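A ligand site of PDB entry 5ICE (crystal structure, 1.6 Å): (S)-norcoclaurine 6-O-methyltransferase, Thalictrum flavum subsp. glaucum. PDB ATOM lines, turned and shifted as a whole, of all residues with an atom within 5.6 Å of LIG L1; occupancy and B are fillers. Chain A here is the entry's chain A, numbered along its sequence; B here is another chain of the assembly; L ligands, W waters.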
ATOM      1  N   GLY A 111      -8.132 -29.276 -15.895  1.00  0.00           N
ATOM      2  CA  GLY A 111      -8.159 -27.876 -15.357  1.00  0.00           C
ATOM      3  C   GLY A 111      -7.732 -26.892 -16.450  1.00  0.00           C
ATOM      4  O   GLY A 111      -8.364 -25.814 -16.590  1.00  0.00           O
ATOM      5  N   ALA A 112      -6.672 -27.238 -17.175  1.00  0.00           N
ATOM      6  CA  ALA A 112      -6.174 -26.364 -18.235  1.00  0.00           C
ATOM      7  C   ALA A 112      -7.217 -26.213 -19.361  1.00  0.00           C
ATOM      8  O   ALA A 112      -7.402 -25.113 -19.909  1.00  0.00           O
ATOM      9  CB  ALA A 112      -4.830 -26.912 -18.770  1.00  0.00           C
ATOM     10  N   THR A 115      -9.963 -23.844 -18.300  1.00  0.00           N
ATOM     11  CA  THR A 115      -9.518 -22.460 -18.305  1.00  0.00           C
ATOM     12  C   THR A 115      -9.423 -21.901 -19.736  1.00  0.00           C
ATOM     13  O   THR A 115      -9.961 -20.831 -20.032  1.00  0.00           O
ATOM     14  CB  THR A 115      -8.095 -22.312 -17.604  1.00  0.00           C
ATOM     15  OG1 THR A 115      -8.231 -22.776 -16.261  1.00  0.00           O
ATOM     16  CG2 THR A 115      -7.615 -20.864 -17.617  1.00  0.00           C
ATOM     17  N   ILE A 116      -8.716 -22.617 -20.593  1.00  0.00           N
ATOM     18  CA  ILE A 116      -8.398 -22.055 -21.890  1.00  0.00           C
ATOM     19  C   ILE A 116      -9.622 -21.945 -22.788  1.00  0.00           C
ATOM     20  O   ILE A 116      -9.745 -20.961 -23.575  1.00  0.00           O
ATOM     21  CB  ILE A 116      -7.309 -22.907 -22.551  1.00  0.00           C
ATOM     22  CG1 ILE A 116      -6.013 -22.786 -21.684  1.00  0.00           C
ATOM     23  CG2 ILE A 116      -6.998 -22.370 -23.999  1.00  0.00           C
ATOM     24  CD1 ILE A 116      -4.916 -23.915 -22.090  1.00  0.00           C
ATOM     25  N   ILE A 150      -5.605  -8.119 -16.981  1.00  0.00           N
ATOM     26  CA  ILE A 150      -5.933  -9.472 -16.480  1.00  0.00           C
ATOM     27  C   ILE A 150      -5.898  -9.547 -14.938  1.00  0.00           C
ATOM     28  O   ILE A 150      -6.750 -10.162 -14.365  1.00  0.00           O
ATOM     29  CB  ILE A 150      -5.032 -10.534 -17.206  1.00  0.00           C
ATOM     30  CG1 ILE A 150      -5.410 -11.928 -16.710  1.00  0.00           C
ATOM     31  CG2 ILE A 150      -3.492 -10.242 -16.955  1.00  0.00           C
ATOM     32  CD1 ILE A 150      -4.841 -13.059 -17.615  1.00  0.00           C
ATOM     33  N   TRP A 151      -4.825  -9.032 -14.315  1.00  0.00           N
ATOM     34  CA  TRP A 151      -4.653  -9.328 -12.863  1.00  0.00           C
ATOM     35  C   TRP A 151      -5.728  -8.561 -12.030  1.00  0.00           C
ATOM     36  O   TRP A 151      -6.247  -9.148 -11.055  1.00  0.00           O
ATOM     37  CB  TRP A 151      -3.240  -8.911 -12.406  1.00  0.00           C
ATOM     38  CG  TRP A 151      -2.175  -9.547 -13.337  1.00  0.00           C
ATOM     39  CD1 TRP A 151      -1.236  -8.863 -14.013  1.00  0.00           C
ATOM     40  CD2 TRP A 151      -2.059 -10.925 -13.723  1.00  0.00           C
ATOM     41  NE1 TRP A 151      -0.462  -9.753 -14.788  1.00  0.00           N
ATOM     42  CE2 TRP A 151      -0.952 -10.994 -14.629  1.00  0.00           C
ATOM     43  CE3 TRP A 151      -2.735 -12.107 -13.383  1.00  0.00           C
ATOM     44  CZ2 TRP A 151      -0.544 -12.217 -15.223  1.00  0.00           C
ATOM     45  CZ3 TRP A 151      -2.355 -13.320 -14.030  1.00  0.00           C
ATOM     46  CH2 TRP A 151      -1.236 -13.337 -14.910  1.00  0.00           C
ATOM     47  N   PHE A 164      -9.007 -19.615 -13.350  1.00  0.00           N
ATOM     48  CA  PHE A 164      -7.673 -19.407 -13.855  1.00  0.00           C
ATOM     49  C   PHE A 164      -6.594 -20.006 -12.947  1.00  0.00           C
ATOM     50  O   PHE A 164      -5.653 -20.670 -13.436  1.00  0.00           O
ATOM     51  CB  PHE A 164      -7.410 -17.890 -14.061  1.00  0.00           C
ATOM     52  CG  PHE A 164      -5.956 -17.586 -14.440  1.00  0.00           C
ATOM     53  CD1 PHE A 164      -5.551 -17.649 -15.795  1.00  0.00           C
ATOM     54  CD2 PHE A 164      -5.009 -17.279 -13.465  1.00  0.00           C
ATOM     55  CE1 PHE A 164      -4.253 -17.377 -16.154  1.00  0.00           C
ATOM     56  CE2 PHE A 164      -3.690 -17.009 -13.813  1.00  0.00           C
ATOM     57  CZ  PHE A 164      -3.306 -17.042 -15.174  1.00  0.00           C
ATOM     58  N   GLY A 167      -6.355 -23.602 -13.487  1.00  0.00           N
ATOM     59  CA  GLY A 167      -5.652 -23.896 -14.747  1.00  0.00           C
ATOM     60  C   GLY A 167      -4.149 -23.874 -14.538  1.00  0.00           C
ATOM     61  O   GLY A 167      -3.419 -24.721 -15.074  1.00  0.00           O
ATOM     62  N   MET A 168      -3.693 -22.849 -13.822  1.00  0.00           N
ATOM     63  CA  MET A 168      -2.274 -22.742 -13.494  1.00  0.00           C
ATOM     64  C   MET A 168      -1.818 -23.887 -12.559  1.00  0.00           C
ATOM     65  O   MET A 168      -0.737 -24.454 -12.761  1.00  0.00           O
ATOM     66  CB  MET A 168      -1.972 -21.389 -12.808  1.00  0.00           C
ATOM     67  CG  MET A 168      -2.233 -20.164 -13.672  1.00  0.00           C
ATOM     68  SD  MET A 168      -1.228 -20.108 -15.201  1.00  0.00           S
ATOM     69  CE  MET A 168      -2.344 -20.811 -16.342  1.00  0.00           C
ATOM     70  N   ASN A 170      -3.041 -26.825 -12.596  1.00  0.00           N
ATOM     71  CA  ASN A 170      -2.917 -27.950 -13.492  1.00  0.00           C
ATOM     72  C   ASN A 170      -1.612 -27.879 -14.259  1.00  0.00           C
ATOM     73  O   ASN A 170      -0.864 -28.841 -14.345  1.00  0.00           O
ATOM     74  CB  ASN A 170      -4.161 -28.014 -14.423  1.00  0.00           C
ATOM     75  CG  ASN A 170      -4.174 -29.276 -15.271  1.00  0.00           C
ATOM     76  OD1 ASN A 170      -3.307 -30.204 -15.160  1.00  0.00           O
ATOM     77  ND2 ASN A 170      -5.192 -29.380 -16.066  1.00  0.00           N
ATOM     78  N   ASP A 171      -1.340 -26.724 -14.893  1.00  0.00           N
ATOM     79  CA  ASP A 171      -0.126 -26.545 -15.672  1.00  0.00           C
ATOM     80  C   ASP A 171       1.124 -26.957 -14.867  1.00  0.00           C
ATOM     81  O   ASP A 171       2.045 -27.577 -15.407  1.00  0.00           O
ATOM     82  CB  ASP A 171       0.004 -25.072 -16.056  1.00  0.00           C
ATOM     83  CG  ASP A 171       0.959 -24.861 -17.277  1.00  0.00           C
ATOM     84  OD1 ASP A 171       0.597 -25.219 -18.391  1.00  0.00           O
ATOM     85  OD2 ASP A 171       2.068 -24.396 -17.027  1.00  0.00           O
ATOM     86  N   LEU A 174       1.604 -30.750 -14.240  1.00  0.00           N
ATOM     87  CA  LEU A 174       2.152 -31.459 -15.412  1.00  0.00           C
ATOM     88  C   LEU A 174       3.681 -31.607 -15.317  1.00  0.00           C
ATOM     89  O   LEU A 174       4.245 -32.534 -15.975  1.00  0.00           O
ATOM     90  CB  LEU A 174       1.796 -30.711 -16.715  1.00  0.00           C
ATOM     91  CG  LEU A 174       0.292 -30.534 -17.003  1.00  0.00           C
ATOM     92  CD1 LEU A 174       0.161 -29.727 -18.301  1.00  0.00           C
ATOM     93  CD2 LEU A 174      -0.487 -31.817 -17.075  1.00  0.00           C
ATOM     94  N   CYS A 255       6.237 -19.466 -15.201  1.00  0.00           N
ATOM     95  CA  CYS A 255       5.191 -18.812 -16.013  1.00  0.00           C
ATOM     96  C   CYS A 255       4.939 -17.392 -15.489  1.00  0.00           C
ATOM     97  O   CYS A 255       3.790 -16.897 -15.540  1.00  0.00           O
ATOM     98  CB  CYS A 255       3.859 -19.654 -15.983  1.00  0.00           C
ATOM     99  SG  CYS A 255       4.103 -21.252 -16.835  1.00  0.00           S
ATOM    100  N   ILE A 256       6.013 -16.735 -15.082  1.00  0.00           N
ATOM    101  CA  ILE A 256       5.966 -15.324 -14.611  1.00  0.00           C
ATOM    102  C   ILE A 256       6.535 -14.403 -15.666  1.00  0.00           C
ATOM    103  O   ILE A 256       5.840 -13.516 -16.164  1.00  0.00           O
ATOM    104  CB  ILE A 256       6.767 -15.151 -13.284  1.00  0.00           C
ATOM    105  CG1 ILE A 256       6.278 -16.123 -12.201  1.00  0.00           C
ATOM    106  CG2 ILE A 256       6.668 -13.651 -12.815  1.00  0.00           C
ATOM    107  CD1 ILE A 256       4.716 -16.053 -11.925  1.00  0.00           C
ATOM    108  N   HIS A 258       7.162 -14.699 -18.748  1.00  0.00           N
ATOM    109  CA  HIS A 258       6.487 -14.622 -20.061  1.00  0.00           C
ATOM    110  C   HIS A 258       5.244 -13.721 -20.021  1.00  0.00           C
ATOM    111  O   HIS A 258       4.693 -13.399 -21.069  1.00  0.00           O
ATOM    112  CB  HIS A 258       6.162 -16.028 -20.584  1.00  0.00           C
ATOM    113  CG  HIS A 258       4.969 -16.658 -19.900  1.00  0.00           C
ATOM    114  ND1 HIS A 258       4.180 -17.611 -20.561  1.00  0.00           N
ATOM    115  CD2 HIS A 258       4.436 -16.523 -18.646  1.00  0.00           C
ATOM    116  CE1 HIS A 258       3.214 -18.003 -19.735  1.00  0.00           C
ATOM    117  NE2 HIS A 258       3.352 -17.360 -18.587  1.00  0.00           N
ATOM    118  N   ASP A 259       4.852 -13.246 -18.826  1.00  0.00           N
ATOM    119  CA  ASP A 259       3.713 -12.272 -18.690  1.00  0.00           C
ATOM    120  C   ASP A 259       4.119 -10.837 -18.964  1.00  0.00           C
ATOM    121  O   ASP A 259       3.242  -9.939 -19.064  1.00  0.00           O
ATOM    122  CB  ASP A 259       3.118 -12.351 -17.282  1.00  0.00           C
ATOM    123  CG  ASP A 259       2.483 -13.647 -16.962  1.00  0.00           C
ATOM    124  OD1 ASP A 259       2.036 -14.396 -17.884  1.00  0.00           O
ATOM    125  OD2 ASP A 259       2.303 -13.940 -15.736  1.00  0.00           O
ATOM    126  N   LEU A 305       1.177 -19.919 -27.357  1.00  0.00           N
ATOM    127  CA  LEU A 305       1.372 -19.164 -26.080  1.00  0.00           C
ATOM    128  C   LEU A 305       1.989 -17.796 -26.261  1.00  0.00           C
ATOM    129  O   LEU A 305       1.737 -16.901 -25.500  1.00  0.00           O
ATOM    130  CB  LEU A 305       2.190 -20.027 -25.092  1.00  0.00           C
ATOM    131  CG  LEU A 305       1.466 -20.772 -24.013  1.00  0.00           C
ATOM    132  CD1 LEU A 305       0.962 -19.823 -22.923  1.00  0.00           C
ATOM    133  CD2 LEU A 305       0.276 -21.554 -24.542  1.00  0.00           C
ATOM    134  N   ASP A 308      -0.927 -15.827 -27.057  1.00  0.00           N
ATOM    135  CA  ASP A 308      -1.754 -15.846 -25.824  1.00  0.00           C
ATOM    136  C   ASP A 308      -1.192 -14.753 -24.888  1.00  0.00           C
ATOM    137  O   ASP A 308      -1.999 -13.951 -24.318  1.00  0.00           O
ATOM    138  CB  ASP A 308      -1.645 -17.227 -25.195  1.00  0.00           C
ATOM    139  CG  ASP A 308      -2.590 -17.413 -23.998  1.00  0.00           C
ATOM    140  OD1 ASP A 308      -2.544 -16.658 -23.032  1.00  0.00           O
ATOM    141  OD2 ASP A 308      -3.423 -18.365 -24.061  1.00  0.00           O
ATOM    142  N   MET A 309       0.113 -14.715 -24.719  1.00  0.00           N
ATOM    143  CA  MET A 309       0.712 -13.635 -23.898  1.00  0.00           C
ATOM    144  C   MET A 309       0.430 -12.271 -24.506  1.00  0.00           C
ATOM    145  O   MET A 309       0.083 -11.319 -23.799  1.00  0.00           O
ATOM    146  CB  MET A 309       2.233 -13.852 -23.731  1.00  0.00           C
ATOM    147  CG  MET A 309       2.598 -15.094 -22.926  1.00  0.00           C
ATOM    148  SD  MET A 309       1.876 -15.115 -21.209  1.00  0.00           S
ATOM    149  CE  MET A 309       0.449 -16.071 -21.471  1.00  0.00           C
ATOM    150  N   ASN A 312      -3.275 -11.511 -23.757  1.00  0.00           N
ATOM    151  CA  ASN A 312      -3.807 -11.560 -22.377  1.00  0.00           C
ATOM    152  C   ASN A 312      -2.990 -10.853 -21.305  1.00  0.00           C
ATOM    153  O   ASN A 312      -3.564 -10.296 -20.388  1.00  0.00           O
ATOM    154  CB  ASN A 312      -3.969 -13.023 -21.963  1.00  0.00           C
ATOM    155  CG  ASN A 312      -5.100 -13.692 -22.721  1.00  0.00           C
ATOM    156  OD1 ASN A 312      -4.895 -14.846 -23.240  1.00  0.00           O
ATOM    157  ND2 ASN A 312      -6.224 -13.116 -22.748  1.00  0.00           N
ATOM    158  N   THR A 313      -1.684 -10.844 -21.452  1.00  0.00           N
ATOM    159  CA  THR A 313      -0.773 -10.325 -20.396  1.00  0.00           C
ATOM    160  C   THR A 313       0.076  -9.165 -20.832  1.00  0.00           C
ATOM    161  O   THR A 313       0.558  -8.371 -19.932  1.00  0.00           O
ATOM    162  CB  THR A 313       0.157 -11.459 -19.863  1.00  0.00           C
ATOM    163  OG1 THR A 313       1.008 -11.917 -20.945  1.00  0.00           O
ATOM    164  CG2 THR A 313      -0.620 -12.634 -19.307  1.00  0.00           C
ATOM    165  N   TRP B  18      -2.907 -30.414 -26.578  1.00  0.00           N
ATOM    166  CA  TRP B  18      -2.722 -28.983 -26.574  1.00  0.00           C
ATOM    167  C   TRP B  18      -3.187 -28.354 -27.909  1.00  0.00           C
ATOM    168  O   TRP B  18      -3.745 -27.268 -27.938  1.00  0.00           O
ATOM    169  CB  TRP B  18      -1.220 -28.639 -26.407  1.00  0.00           C
ATOM    170  CG  TRP B  18      -0.720 -28.788 -24.990  1.00  0.00           C
ATOM    171  CD1 TRP B  18       0.328 -29.608 -24.577  1.00  0.00           C
ATOM    172  CD2 TRP B  18      -1.144 -28.037 -23.853  1.00  0.00           C
ATOM    173  NE1 TRP B  18       0.510 -29.448 -23.197  1.00  0.00           N
ATOM    174  CE2 TRP B  18      -0.347 -28.482 -22.742  1.00  0.00           C
ATOM    175  CE3 TRP B  18      -2.143 -27.083 -23.635  1.00  0.00           C
ATOM    176  CZ2 TRP B  18      -0.518 -27.998 -21.446  1.00  0.00           C
ATOM    177  CZ3 TRP B  18      -2.325 -26.567 -22.315  1.00  0.00           C
ATOM    178  CH2 TRP B  18      -1.511 -27.032 -21.217  1.00  0.00           C
ATOM    179  N   TYR B  22      -6.211 -25.601 -28.238  1.00  0.00           N
ATOM    180  CA  TYR B  22      -5.988 -24.287 -28.908  1.00  0.00           C
ATOM    181  C   TYR B  22      -6.426 -24.268 -30.337  1.00  0.00           C
ATOM    182  O   TYR B  22      -5.957 -23.427 -31.135  1.00  0.00           O
ATOM    183  CB  TYR B  22      -4.536 -23.878 -28.772  1.00  0.00           C
ATOM    184  CG  TYR B  22      -4.209 -23.183 -27.474  1.00  0.00           C
ATOM    185  CD1 TYR B  22      -4.653 -21.871 -27.246  1.00  0.00           C
ATOM    186  CD2 TYR B  22      -3.404 -23.810 -26.481  1.00  0.00           C
ATOM    187  CE1 TYR B  22      -4.319 -21.206 -26.072  1.00  0.00           C
ATOM    188  CE2 TYR B  22      -3.059 -23.135 -25.288  1.00  0.00           C
ATOM    189  CZ  TYR B  22      -3.537 -21.845 -25.092  1.00  0.00           C
ATOM    190  OH  TYR B  22      -3.198 -21.162 -23.940  1.00  0.00           O
HETATM  191  O1  LIG L   1       0.939 -16.629 -16.973  1.00  0.00           O
HETATM  192  C1  LIG L   1      -0.101 -17.127 -17.760  1.00  0.00           C
HETATM  193  C2  LIG L   1      -1.095 -16.274 -18.173  1.00  0.00           C
HETATM  194  C3  LIG L   1      -0.032 -18.442 -18.168  1.00  0.00           C
HETATM  195  O2  LIG L   1       1.012 -19.279 -17.779  1.00  0.00           O
HETATM  196  C4  LIG L   1      -1.072 -18.973 -18.972  1.00  0.00           C
HETATM  197  C5  LIG L   1      -2.098 -18.123 -19.357  1.00  0.00           C
HETATM  198  C6  LIG L   1      -2.162 -16.781 -18.982  1.00  0.00           C
HETATM  199  C7  LIG L   1      -3.243 -15.832 -19.434  1.00  0.00           C
HETATM  200  C8  LIG L   1      -4.423 -16.509 -20.042  1.00  0.00           C
HETATM  201  N1  LIG L   1      -3.988 -17.614 -20.985  1.00  0.00           N
HETATM  202  C9  LIG L   1      -3.288 -18.683 -20.202  1.00  0.00           C
HETATM  203  C10 LIG L   1      -3.068 -19.851 -21.042  1.00  0.00           C
HETATM  204  C11 LIG L   1      -2.857 -21.267 -20.313  1.00  0.00           C
HETATM  205  C12 LIG L   1      -3.685 -21.649 -19.273  1.00  0.00           C
HETATM  206  C13 LIG L   1      -1.838 -22.024 -20.736  1.00  0.00           C
HETATM  207  C14 LIG L   1      -1.574 -23.250 -20.138  1.00  0.00           C
HETATM  208  C15 LIG L   1      -2.360 -23.685 -19.096  1.00  0.00           C
HETATM  209  O3  LIG L   1      -2.092 -24.912 -18.489  1.00  0.00           O
HETATM  210  C16 LIG L   1      -3.424 -22.917 -18.636  1.00  0.00           C
HETATM  211  O4  LIG L   1      -4.247 -23.405 -17.652  1.00  0.00           O
HETATM  212  N1  LG2 L   2       3.532 -19.704 -10.999  1.00  0.00           N
HETATM  213  C1  LG2 L   2       2.126 -20.209 -11.178  1.00  0.00           C
HETATM  214  C2  LG2 L   2       1.199 -19.123 -11.767  1.00  0.00           C
HETATM  215  C3  LG2 L   2       1.678 -18.531 -13.076  1.00  0.00           C
HETATM  216  S1  LG2 L   2       0.477 -17.294 -13.675  1.00  0.00           S
HETATM  217  C4  LG2 L   2       2.157 -21.368 -12.145  1.00  0.00           C
HETATM  218  O1  LG2 L   2       1.252 -22.216 -12.081  1.00  0.00           O
HETATM  219  O2  LG2 L   2       3.081 -21.525 -12.980  1.00  0.00           O
HETATM  220  C5  LG2 L   2       1.184 -15.736 -13.191  1.00  0.00           C
HETATM  221  C6  LG2 L   2       1.040 -15.502 -11.679  1.00  0.00           C
HETATM  222  O3  LG2 L   2       1.759 -14.241 -11.360  1.00  0.00           O
HETATM  223  C7  LG2 L   2      -0.404 -15.294 -11.234  1.00  0.00           C
HETATM  224  O4  LG2 L   2      -0.637 -16.212 -10.117  1.00  0.00           O
HETATM  225  C8  LG2 L   2      -0.486 -13.847 -10.795  1.00  0.00           C
HETATM  226  O5  LG2 L   2      -1.402 -13.617  -9.744  1.00  0.00           O
HETATM  227  C9  LG2 L   2       0.938 -13.509 -10.382  1.00  0.00           C
HETATM  228  N2  LG2 L   2       1.236 -12.108 -10.409  1.00  0.00           N
HETATM  229  C10 LG2 L   2       0.903 -11.180 -11.323  1.00  0.00           C
HETATM  230  N3  LG2 L   2       1.353  -9.972 -10.985  1.00  0.00           N
HETATM  231  C11 LG2 L   2       1.980 -10.094  -9.780  1.00  0.00           C
HETATM  232  C12 LG2 L   2       2.696  -9.158  -8.852  1.00  0.00           C
HETATM  233  N4  LG2 L   2       2.791  -7.862  -9.147  1.00  0.00           N
HETATM  234  N5  LG2 L   2       3.220  -9.708  -7.764  1.00  0.00           N
HETATM  235  C13 LG2 L   2       3.109 -11.027  -7.454  1.00  0.00           C
HETATM  236  N6  LG2 L   2       2.447 -11.939  -8.233  1.00  0.00           N
HETATM  237  C14 LG2 L   2       1.928 -11.476  -9.410  1.00  0.00           C
HETATM  238  O   HOH W   1      -6.639 -18.654 -20.963  1.00  0.00           O
HETATM  239  O   HOH W   2      -7.396 -16.474 -19.199  1.00  0.00           O
HETATM  240  O   HOH W   3       1.712 -22.475 -20.896  1.00  0.00           O
HETATM  241  O   HOH W   4       0.866 -21.740 -18.397  1.00  0.00           O
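O1 of LIG L1 lies within hydrogen-bond range of OD1 of Asp 259 (2.6 Å).
A nitrogen (N1) of LIG L1 is in salt-bridge range of the side-chain carboxylate of Asp 308, at 2.7 Å.
The side-chain carboxylate of Asp 171 lies within hydrogen-bond range of an oxygen (O3) of LIG L1 (2.7 Å).
A ring nitrogen (NE2) of His 258 is in hydrogen-bond range of an oxygen (O1) of LIG L1, at 3.0 Å.
An oxygen (O4) of LIG L1 lies within hydrogen-bond range of the backbone carbonyl oxygen (O) of Gly 167 (3.0 Å).
The backbone carbonyl oxygen (O) of Cys 255 lies within hydrogen-bond range of an oxygen (O1) of LIG L1, 3.2 Å away.
The side-chain sulfur (SG) of Cys 255 lies close to an oxygen (O2) of LIG L1, 3.8 Å away.
O2 of LIG L1 lies within hydrogen-bond range of SD of Met 168 (3.5 Å).
An oxygen (O1) of LG2 L2 lies close to the backbone carbonyl oxygen of Met 168 (3.1 Å).
A sulfur (S1) of LG2 L2 lies close to an oxygen (O1) of LIG L1 (3.4 Å).
CB of Ala 112 touches O3 of LIG L1, at 3.4 Å.
Ile 116 touches LIG L1.
CD1 of Ile 150 touches C7 of LIG L1, 3.7 Å away.
Phe 164 touches LIG L1.
CE of Met 309 touches C2 of LIG L1, at 3.6 Å.
Asn 312 touches LIG L1 (OD1 to C8, 3.6 Å).
Thr 313 touches LIG L1 (CG2 to C2, 3.8 Å).
Trp 18 of chain B touches LIG L1 (CH2 to O3, 3.5 Å).
Tyr 22 of chain B touches LIG L1.
Of the 23 residues printed, 16 come within 4 Å of LIG L1.
The nearest printed residue that does not touch LIG L1 is Thr 115 (4.001 Å).
OD1 of Asp 259 lies close to NE2 of His 258, 3.3 Å away.
The side-chain carboxylate (OD2) of Asp 308 is in hydrogen-bond range of the side-chain hydroxyl (OH) of Tyr 22 of chain B.
OD1 of Asn 312 lies close to OD1 of Asp 308 (3.0 Å).
The side-chain carboxylate of Asp 171 is in hydrogen-bond range of the side-chain sulfur of Cys 255.
NE2 of His 258 sits at hydrogen-bond distance from O of Cys 255, 3.1 Å away.
A ring nitrogen (ND1) of His 258 lies within hydrogen-bond range of the side-chain sulfur (SD) of Met 309 (3.5 Å).
ND2 of Asn 170 lies close to N of Ala 112 (2.8 Å).
The side-chain hydroxyl of Thr 313 is in hydrogen-bond range of the backbone carbonyl oxygen of Met 309, 3.1 Å away.
Water W4 lies within hydrogen-bond range of O2 of LIG L1, OD2 of Asp 171 and SG of Cys 255.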
